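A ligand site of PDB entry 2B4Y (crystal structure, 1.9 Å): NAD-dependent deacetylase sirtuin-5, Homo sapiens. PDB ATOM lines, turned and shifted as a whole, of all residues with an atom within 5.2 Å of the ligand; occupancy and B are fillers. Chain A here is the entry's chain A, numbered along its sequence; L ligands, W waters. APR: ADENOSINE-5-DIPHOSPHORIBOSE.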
ATOM      1  N   SER A  26      18.640 -10.476  13.922  1.00  0.00           N
ATOM      2  CA  SER A  26      18.972 -10.553  12.540  1.00  0.00           C
ATOM      3  C   SER A  26      18.852 -11.982  11.955  1.00  0.00           C
ATOM      4  O   SER A  26      18.964 -12.987  12.690  1.00  0.00           O
ATOM      5  CB  SER A  26      20.362  -9.967  12.265  1.00  0.00           C
ATOM      6  OG  SER A  26      21.380 -10.746  12.854  1.00  0.00           O
ATOM      7  N   GLY A  27      18.578 -12.025  10.642  1.00  0.00           N
ATOM      8  CA  GLY A  27      18.606 -13.258   9.859  1.00  0.00           C
ATOM      9  C   GLY A  27      19.340 -13.102   8.555  1.00  0.00           C
ATOM     10  O   GLY A  27      20.107 -12.131   8.314  1.00  0.00           O
ATOM     11  N   ALA A  28      19.074 -14.050   7.659  1.00  0.00           N
ATOM     12  CA  ALA A  28      19.855 -14.119   6.443  1.00  0.00           C
ATOM     13  C   ALA A  28      19.814 -12.898   5.549  1.00  0.00           C
ATOM     14  O   ALA A  28      20.788 -12.626   4.858  1.00  0.00           O
ATOM     15  CB  ALA A  28      19.537 -15.358   5.663  1.00  0.00           C
ATOM     16  N   GLY A  29      18.717 -12.118   5.618  1.00  0.00           N
ATOM     17  CA  GLY A  29      18.579 -10.911   4.823  1.00  0.00           C
ATOM     18  C   GLY A  29      19.668  -9.890   5.081  1.00  0.00           C
ATOM     19  O   GLY A  29      20.045  -9.127   4.186  1.00  0.00           O
ATOM     20  N   VAL A  30      20.182  -9.864   6.324  1.00  0.00           N
ATOM     21  CA  VAL A  30      21.230  -8.891   6.707  1.00  0.00           C
ATOM     22  C   VAL A  30      22.563  -9.139   5.978  1.00  0.00           C
ATOM     23  O   VAL A  30      23.380  -8.231   5.806  1.00  0.00           O
ATOM     24  CB  VAL A  30      21.369  -8.813   8.283  1.00  0.00           C
ATOM     25  CG1 VAL A  30      22.360  -9.858   8.808  1.00  0.00           C
ATOM     26  CG2 VAL A  30      21.753  -7.442   8.716  1.00  0.00           C
ATOM     27  N   ALA A  32      22.625 -10.555   2.771  1.00  0.00           N
ATOM     28  CA  ALA A  32      22.306 -10.605   1.329  1.00  0.00           C
ATOM     29  C   ALA A  32      23.189  -9.657   0.555  1.00  0.00           C
ATOM     30  O   ALA A  32      23.715 -10.002  -0.487  1.00  0.00           O
ATOM     31  CB  ALA A  32      20.864 -10.252   1.115  1.00  0.00           C
ATOM     32  N   GLU A  33      23.374  -8.449   1.077  1.00  0.00           N
ATOM     33  CA  GLU A  33      24.190  -7.429   0.376  1.00  0.00           C
ATOM     34  C   GLU A  33      25.703  -7.658   0.521  1.00  0.00           C
ATOM     35  O   GLU A  33      26.518  -6.895  -0.027  1.00  0.00           O
ATOM     36  CB  GLU A  33      23.776  -6.034   0.854  1.00  0.00           C
ATOM     37  CG  GLU A  33      22.290  -5.716   0.568  1.00  0.00           C
ATOM     38  CD  GLU A  33      21.779  -4.488   1.271  1.00  0.00           C
ATOM     39  OE1 GLU A  33      22.207  -3.375   0.912  1.00  0.00           O
ATOM     40  OE2 GLU A  33      20.918  -4.620   2.189  1.00  0.00           O
ATOM     41  N   GLN A 109      20.550 -15.317  13.892  1.00  0.00           N
ATOM     42  CA  GLN A 109      20.265 -16.649  13.464  1.00  0.00           C
ATOM     43  C   GLN A 109      21.357 -17.122  12.511  1.00  0.00           C
ATOM     44  O   GLN A 109      21.439 -18.295  12.240  1.00  0.00           O
ATOM     45  CB  GLN A 109      18.921 -16.624  12.731  1.00  0.00           C
ATOM     46  CG  GLN A 109      17.725 -16.542  13.676  1.00  0.00           C
ATOM     47  CD  GLN A 109      16.436 -16.165  12.957  1.00  0.00           C
ATOM     48  OE1 GLN A 109      16.146 -14.970  12.684  1.00  0.00           O
ATOM     49  NE2 GLN A 109      15.623 -17.180  12.697  1.00  0.00           N
ATOM     50  N   ASN A 110      22.161 -16.196  12.017  1.00  0.00           N
ATOM     51  CA  ASN A 110      23.212 -16.461  11.036  1.00  0.00           C
ATOM     52  C   ASN A 110      24.481 -17.099  11.663  1.00  0.00           C
ATOM     53  O   ASN A 110      24.826 -16.789  12.790  1.00  0.00           O
ATOM     54  CB  ASN A 110      23.623 -15.140  10.363  1.00  0.00           C
ATOM     55  CG  ASN A 110      22.442 -14.393   9.765  1.00  0.00           C
ATOM     56  OD1 ASN A 110      21.462 -15.009   9.380  1.00  0.00           O
ATOM     57  ND2 ASN A 110      22.539 -13.045   9.678  1.00  0.00           N
ATOM     58  N   HIS A 127      22.290 -20.065  16.616  1.00  0.00           N
ATOM     59  CA  HIS A 127      22.481 -21.284  15.817  1.00  0.00           C
ATOM     60  C   HIS A 127      23.914 -21.753  15.707  1.00  0.00           C
ATOM     61  O   HIS A 127      24.209 -22.593  14.850  1.00  0.00           O
ATOM     62  CB  HIS A 127      21.903 -21.133  14.372  1.00  0.00           C
ATOM     63  CG  HIS A 127      20.412 -20.967  14.322  1.00  0.00           C
ATOM     64  ND1 HIS A 127      19.791 -20.154  13.409  1.00  0.00           N
ATOM     65  CD2 HIS A 127      19.435 -21.504  15.082  1.00  0.00           C
ATOM     66  CE1 HIS A 127      18.486 -20.205  13.587  1.00  0.00           C
ATOM     67  NE2 HIS A 127      18.245 -21.015  14.599  1.00  0.00           N
ATOM     68  N   PHE A 192      19.518 -29.416  11.656  1.00  0.00           N
ATOM     69  CA  PHE A 192      18.076 -29.717  11.613  1.00  0.00           C
ATOM     70  C   PHE A 192      17.800 -30.880  12.550  1.00  0.00           C
ATOM     71  O   PHE A 192      18.513 -31.896  12.541  1.00  0.00           O
ATOM     72  CB  PHE A 192      17.638 -30.083  10.170  1.00  0.00           C
ATOM     73  CG  PHE A 192      17.595 -28.899   9.202  1.00  0.00           C
ATOM     74  CD1 PHE A 192      16.483 -28.051   9.148  1.00  0.00           C
ATOM     75  CD2 PHE A 192      18.657 -28.654   8.343  1.00  0.00           C
ATOM     76  CE1 PHE A 192      16.447 -26.958   8.235  1.00  0.00           C
ATOM     77  CE2 PHE A 192      18.635 -27.567   7.422  1.00  0.00           C
ATOM     78  CZ  PHE A 192      17.523 -26.719   7.368  1.00  0.00           C
ATOM     79  N   GLY A 218      16.091  -8.431   8.256  1.00  0.00           N
ATOM     80  CA  GLY A 218      16.239  -9.491   7.292  1.00  0.00           C
ATOM     81  C   GLY A 218      15.851 -10.885   7.769  1.00  0.00           C
ATOM     82  O   GLY A 218      16.582 -11.847   7.584  1.00  0.00           O
ATOM     83  N   THR A 219      14.723 -11.012   8.419  1.00  0.00           N
ATOM     84  CA  THR A 219      14.284 -12.350   8.771  1.00  0.00           C
ATOM     85  C   THR A 219      12.829 -12.590   8.322  1.00  0.00           C
ATOM     86  O   THR A 219      12.009 -11.676   8.323  1.00  0.00           O
ATOM     87  CB  THR A 219      14.570 -12.691  10.253  1.00  0.00           C
ATOM     88  OG1 THR A 219      14.068 -13.995  10.568  1.00  0.00           O
ATOM     89  CG2 THR A 219      13.961 -11.672  11.175  1.00  0.00           C
ATOM     90  N   SER A 220      12.533 -13.833   7.967  1.00  0.00           N
ATOM     91  CA  SER A 220      11.221 -14.222   7.400  1.00  0.00           C
ATOM     92  C   SER A 220      10.195 -14.313   8.492  1.00  0.00           C
ATOM     93  O   SER A 220       9.001 -14.294   8.181  1.00  0.00           O
ATOM     94  CB  SER A 220      11.298 -15.542   6.629  1.00  0.00           C
ATOM     95  OG  SER A 220      11.679 -16.647   7.466  1.00  0.00           O
ATOM     96  N   SER A 221      10.671 -14.401   9.758  1.00  0.00           N
ATOM     97  CA  SER A 221       9.816 -14.505  10.953  1.00  0.00           C
ATOM     98  C   SER A 221       8.836 -15.691  10.962  1.00  0.00           C
ATOM     99  O   SER A 221       7.702 -15.571  11.481  1.00  0.00           O
ATOM    100  CB  SER A 221       9.057 -13.201  11.211  1.00  0.00           C
ATOM    101  OG  SER A 221       9.890 -12.211  11.748  1.00  0.00           O
ATOM    102  N   VAL A 223      10.404 -19.154  11.159  1.00  0.00           N
ATOM    103  CA  VAL A 223      11.206 -20.223  11.783  1.00  0.00           C
ATOM    104  C   VAL A 223      11.389 -20.025  13.331  1.00  0.00           C
ATOM    105  O   VAL A 223      11.875 -18.990  13.822  1.00  0.00           O
ATOM    106  CB  VAL A 223      12.545 -20.443  11.008  1.00  0.00           C
ATOM    107  CG1 VAL A 223      13.330 -21.646  11.569  1.00  0.00           C
ATOM    108  CG2 VAL A 223      12.201 -20.638   9.499  1.00  0.00           C
ATOM    109  N   PHE A 243      12.820  -4.350   9.495  1.00  0.00           N
ATOM    110  CA  PHE A 243      13.555  -3.880   8.345  1.00  0.00           C
ATOM    111  C   PHE A 243      13.666  -5.088   7.429  1.00  0.00           C
ATOM    112  O   PHE A 243      14.386  -6.023   7.745  1.00  0.00           O
ATOM    113  CB  PHE A 243      14.971  -3.380   8.765  1.00  0.00           C
ATOM    114  CG  PHE A 243      14.951  -2.106   9.592  1.00  0.00           C
ATOM    115  CD1 PHE A 243      15.257  -0.891   9.025  1.00  0.00           C
ATOM    116  CD2 PHE A 243      14.688  -2.135  10.949  1.00  0.00           C
ATOM    117  CE1 PHE A 243      15.235   0.336   9.788  1.00  0.00           C
ATOM    118  CE2 PHE A 243      14.658  -0.937  11.709  1.00  0.00           C
ATOM    119  CZ  PHE A 243      14.942   0.278  11.130  1.00  0.00           C
ATOM    120  N   ASN A 244      12.950  -5.074   6.299  1.00  0.00           N
ATOM    121  CA  ASN A 244      12.886  -6.215   5.414  1.00  0.00           C
ATOM    122  C   ASN A 244      12.569  -5.705   3.982  1.00  0.00           C
ATOM    123  O   ASN A 244      11.938  -4.670   3.825  1.00  0.00           O
ATOM    124  CB  ASN A 244      11.784  -7.189   5.891  1.00  0.00           C
ATOM    125  CG  ASN A 244      11.969  -8.617   5.320  1.00  0.00           C
ATOM    126  OD1 ASN A 244      11.963  -8.829   4.111  1.00  0.00           O
ATOM    127  ND2 ASN A 244      12.155  -9.591   6.216  1.00  0.00           N
ATOM    128  N   THR A 245      13.011  -6.429   2.961  1.00  0.00           N
ATOM    129  CA  THR A 245      12.620  -6.131   1.575  1.00  0.00           C
ATOM    130  C   THR A 245      11.139  -6.379   1.283  1.00  0.00           C
ATOM    131  O   THR A 245      10.604  -5.857   0.296  1.00  0.00           O
ATOM    132  CB  THR A 245      13.465  -6.947   0.584  1.00  0.00           C
ATOM    133  OG1 THR A 245      13.616  -8.275   1.083  1.00  0.00           O
ATOM    134  CG2 THR A 245      14.822  -6.342   0.420  1.00  0.00           C
ATOM    135  N   GLU A 246      10.471  -7.173   2.123  1.00  0.00           N
ATOM    136  CA  GLU A 246       9.048  -7.524   1.954  1.00  0.00           C
ATOM    137  C   GLU A 246       8.289  -7.471   3.255  1.00  0.00           C
ATOM    138  O   GLU A 246       8.875  -7.547   4.322  1.00  0.00           O
ATOM    139  CB  GLU A 246       8.952  -8.974   1.520  1.00  0.00           C
ATOM    140  CG  GLU A 246       9.401  -9.226   0.102  1.00  0.00           C
ATOM    141  CD  GLU A 246      10.229 -10.459   0.026  1.00  0.00           C
ATOM    142  OE1 GLU A 246       9.628 -11.555   0.217  1.00  0.00           O
ATOM    143  OE2 GLU A 246      11.478 -10.326  -0.210  1.00  0.00           O
ATOM    144  N   THR A 248       6.259  -9.613   5.997  1.00  0.00           N
ATOM    145  CA  THR A 248       6.316 -10.975   6.436  1.00  0.00           C
ATOM    146  C   THR A 248       5.018 -11.242   7.157  1.00  0.00           C
ATOM    147  O   THR A 248       4.231 -10.302   7.385  1.00  0.00           O
ATOM    148  CB  THR A 248       7.541 -11.242   7.400  1.00  0.00           C
ATOM    149  OG1 THR A 248       7.307 -10.598   8.635  1.00  0.00           O
ATOM    150  CG2 THR A 248       8.838 -10.708   6.768  1.00  0.00           C
ATOM    151  N   GLY A 260      12.772  -2.212   2.193  1.00  0.00           N
ATOM    152  CA  GLY A 260      13.915  -1.897   1.417  1.00  0.00           C
ATOM    153  C   GLY A 260      15.084  -2.774   1.850  1.00  0.00           C
ATOM    154  O   GLY A 260      15.001  -3.505   2.873  1.00  0.00           O
ATOM    155  N   PRO A 261      16.187  -2.718   1.091  1.00  0.00           N
ATOM    156  CA  PRO A 261      17.365  -3.462   1.501  1.00  0.00           C
ATOM    157  C   PRO A 261      17.924  -2.801   2.785  1.00  0.00           C
ATOM    158  O   PRO A 261      18.037  -1.589   2.847  1.00  0.00           O
ATOM    159  CB  PRO A 261      18.319  -3.343   0.304  1.00  0.00           C
ATOM    160  CG  PRO A 261      17.864  -2.131  -0.448  1.00  0.00           C
ATOM    161  CD  PRO A 261      16.395  -1.929  -0.140  1.00  0.00           C
ATOM    162  N   CYS A 262      18.229  -3.596   3.806  1.00  0.00           N
ATOM    163  CA  CYS A 262      18.688  -3.054   5.094  1.00  0.00           C
ATOM    164  C   CYS A 262      20.000  -2.285   5.021  1.00  0.00           C
ATOM    165  O   CYS A 262      20.306  -1.499   5.912  1.00  0.00           O
ATOM    166  CB  CYS A 262      18.671  -4.154   6.188  1.00  0.00           C
ATOM    167  SG  CYS A 262      19.907  -5.424   6.039  1.00  0.00           S
ATOM    168  N   GLY A 263      20.782  -2.472   3.955  1.00  0.00           N
ATOM    169  CA  GLY A 263      21.979  -1.669   3.737  1.00  0.00           C
ATOM    170  C   GLY A 263      21.683  -0.238   3.366  1.00  0.00           C
ATOM    171  O   GLY A 263      22.561   0.621   3.415  1.00  0.00           O
HETATM  172  N1  APR L   1      17.561  -6.490   3.483  1.00  0.00           N
HETATM  173  C2  APR L   1      16.626  -6.864   4.382  1.00  0.00           C
HETATM  174  N3  APR L   1      15.954  -8.033   4.294  1.00  0.00           N
HETATM  175  C4  APR L   1      16.196  -8.905   3.264  1.00  0.00           C
HETATM  176  C5  APR L   1      17.207  -8.580   2.261  1.00  0.00           C
HETATM  177  C6  APR L   1      17.889  -7.277   2.424  1.00  0.00           C
HETATM  178  N6  APR L   1      18.826  -6.845   1.557  1.00  0.00           N
HETATM  179  N7  APR L   1      17.251  -9.619   1.384  1.00  0.00           N
HETATM  180  C8  APR L   1      16.346 -10.539   1.791  1.00  0.00           C
HETATM  181  N9  APR L   1      15.724 -10.122   2.931  1.00  0.00           N
HETATM  182  C1' APR L   1      14.710 -10.814   3.707  1.00  0.00           C
HETATM  183  C2' APR L   1      13.705 -11.662   2.910  1.00  0.00           C
HETATM  184  O2' APR L   1      12.715 -10.724   2.525  1.00  0.00           O
HETATM  185  C3' APR L   1      13.265 -12.646   3.969  1.00  0.00           C
HETATM  186  O3' APR L   1      12.193 -12.135   4.794  1.00  0.00           O
HETATM  187  O4' APR L   1      15.379 -11.697   4.608  1.00  0.00           O
HETATM  188  C4' APR L   1      14.484 -12.764   4.910  1.00  0.00           C
HETATM  189  C5' APR L   1      15.280 -14.028   4.672  1.00  0.00           C
HETATM  190  O5' APR L   1      14.511 -15.068   5.237  1.00  0.00           O
HETATM  191  PA  APR L   1      15.098 -16.548   5.374  1.00  0.00           P
HETATM  192  O1A APR L   1      15.946 -16.865   4.178  1.00  0.00           O
HETATM  193  O2A APR L   1      13.892 -17.358   5.845  1.00  0.00           O
HETATM  194  O3A APR L   1      16.214 -16.364   6.557  1.00  0.00           O
HETATM  195  PB  APR L   1      16.083 -16.374   8.157  1.00  0.00           P
HETATM  196  O1B APR L   1      14.801 -15.745   8.629  1.00  0.00           O
HETATM  197  O2B APR L   1      17.389 -16.018   8.834  1.00  0.00           O
HETATM  198  O5D APR L   1      15.857 -17.955   8.357  1.00  0.00           O
HETATM  199  C5D APR L   1      15.697 -18.501   9.656  1.00  0.00           C
HETATM  200  O4D APR L   1      15.962 -20.750   8.780  1.00  0.00           O
HETATM  201  O1D APR L   1      16.871 -21.825   6.959  1.00  0.00           O
HETATM  202  C1D APR L   1      16.973 -21.662   8.400  1.00  0.00           C
HETATM  203  O2D APR L   1      18.909 -21.758   9.825  1.00  0.00           O
HETATM  204  C2D APR L   1      18.299 -21.011   8.774  1.00  0.00           C
HETATM  205  O3D APR L   1      18.741 -19.399  10.517  1.00  0.00           O
HETATM  206  C3D APR L   1      17.929 -19.684   9.375  1.00  0.00           C
HETATM  207  C4D APR L   1      16.463 -19.833   9.742  1.00  0.00           C
HETATM  208  O   HOH W   1      14.836 -20.094   6.422  1.00  0.00           O
HETATM  209  O   HOH W   2      21.863  -7.377   3.179  1.00  0.00           O
HETATM  210  O   HOH W   3      21.599 -20.554  10.394  1.00  0.00           O
HETATM  211  O   HOH W   4      19.666 -17.130   9.319  1.00  0.00           O
HETATM  212  O   HOH W   5      12.072 -17.199   9.869  1.00  0.00           O
HETATM  213  O   HOH W   6       9.694 -12.950   3.932  1.00  0.00           O
HETATM  214  O   HOH W   7      18.457 -10.010  -1.308  1.00  0.00           O
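The side-chain amide oxygen (OD1) of Asn 244 lies within hydrogen-bond range of an oxygen (O2') of the ligand. OG1 of Thr 219 sits at hydrogen-bond distance from O1B of the ligand (2.7 Å). N of Ser 220 sits at hydrogen-bond distance from O1B of the ligand (3.0 Å). An oxygen (O2A) of the ligand is in hydrogen-bond range of the side-chain hydroxyl of Ser 220, 2.8 Å away. The backbone NH (N) of Ala 28 sits at hydrogen-bond distance from an oxygen (O2B) of the ligand. The side-chain hydroxyl (OG1) of Thr 245 sits at hydrogen-bond distance from an oxygen (O2') of the ligand, 3.0 Å away. The backbone NH (N) of Cys 262 lies within hydrogen-bond range of a nitrogen (N1) of the ligand (3.0 Å). The side-chain sulfur (SG) of Cys 262 sits at hydrogen-bond distance from a nitrogen (N1) of the ligand. The side-chain carboxylate (OE2) of Glu 246 lies within hydrogen-bond range of an oxygen (O2') of the ligand (3.0 Å). OE2 of Glu 33 sits at hydrogen-bond distance from N6 of the ligand (3.1 Å). ND1 of His 127 sits at hydrogen-bond distance from O3D of the ligand, at 3.2 Å. O3D of the ligand sits at hydrogen-bond distance from O of Gln 109, at 3.4 Å.
ND2 of Asn 244 lies within hydrogen-bond range of O of Thr 219 (3.0 Å). OD1 of Asn 244 lies within hydrogen-bond range of N of Glu 246, at 3.0 Å. The side-chain hydroxyl (OG1) of Thr 219 is in hydrogen-bond range of the side-chain amide oxygen (OE1) of Gln 109, 3.1 Å away. O of Gly 218 is in hydrogen-bond range of N of Ala 28. N of Ala 28 lies within hydrogen-bond range of OD1 of Asn 110. OG1 of Thr 245 is in hydrogen-bond range of OE2 of Glu 246. The side-chain carboxylate (OE2) of Glu 33 lies within hydrogen-bond range of the backbone NH (N) of Gly 263 (2.8 Å). O of Gly 218 is in hydrogen-bond range of N of Gly 29 (2.9 Å).
O of Gly 218 lies close to O4' of the ligand, 3.2 Å away. Gly 27 touches the ligand. Gly 29 touches the ligand (CA to O4', 3.3 Å). Ala 32 touches the ligand (CB to N7, 3.7 Å). Val 223 touches the ligand. O of Gly 260 touches N1 of the ligand, 3.98 Å away. CA of Pro 261 touches N1 of the ligand, 3.6 Å away. Hydrophobic or aromatic side chains that line the ligand: Ala 28, Ala 32, His 127, Val 223 and Pro 261. Within 4 Å of the ligand: Gly 27, Ala 28, Gly 29, Ala 32, Glu 33, Gln 109, His 127, Gly 218, Thr 219, Ser 220, Val 223, Asn 244, Thr 245, Glu 246, Gly 260, Pro 261 and Cys 262. Along chain A the residues within 4 Å of the ligand span positions 27 to 262. The nearest printed residue that does not touch the ligand is Phe 243 (4.1 Å).
Water W4 lies within hydrogen-bond range of O2B of the ligand (2.6 Å) and OD1 of Asn 110 (2.8 Å). Water W3 lies within hydrogen-bond range of the backbone carbonyl oxygen (O) of Gln 109 (2.9 Å) and an oxygen (O2D) of the ligand (3.0 Å). Water W5 lies within hydrogen-bond range of the side-chain hydroxyl (OG) of Ser 220 (2.5 Å), the backbone NH (N) of Val 223 (2.9 Å), the backbone NH (N) of Ser 221 (3.1 Å) and an oxygen (O1B) of the ligand (3.3 Å).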
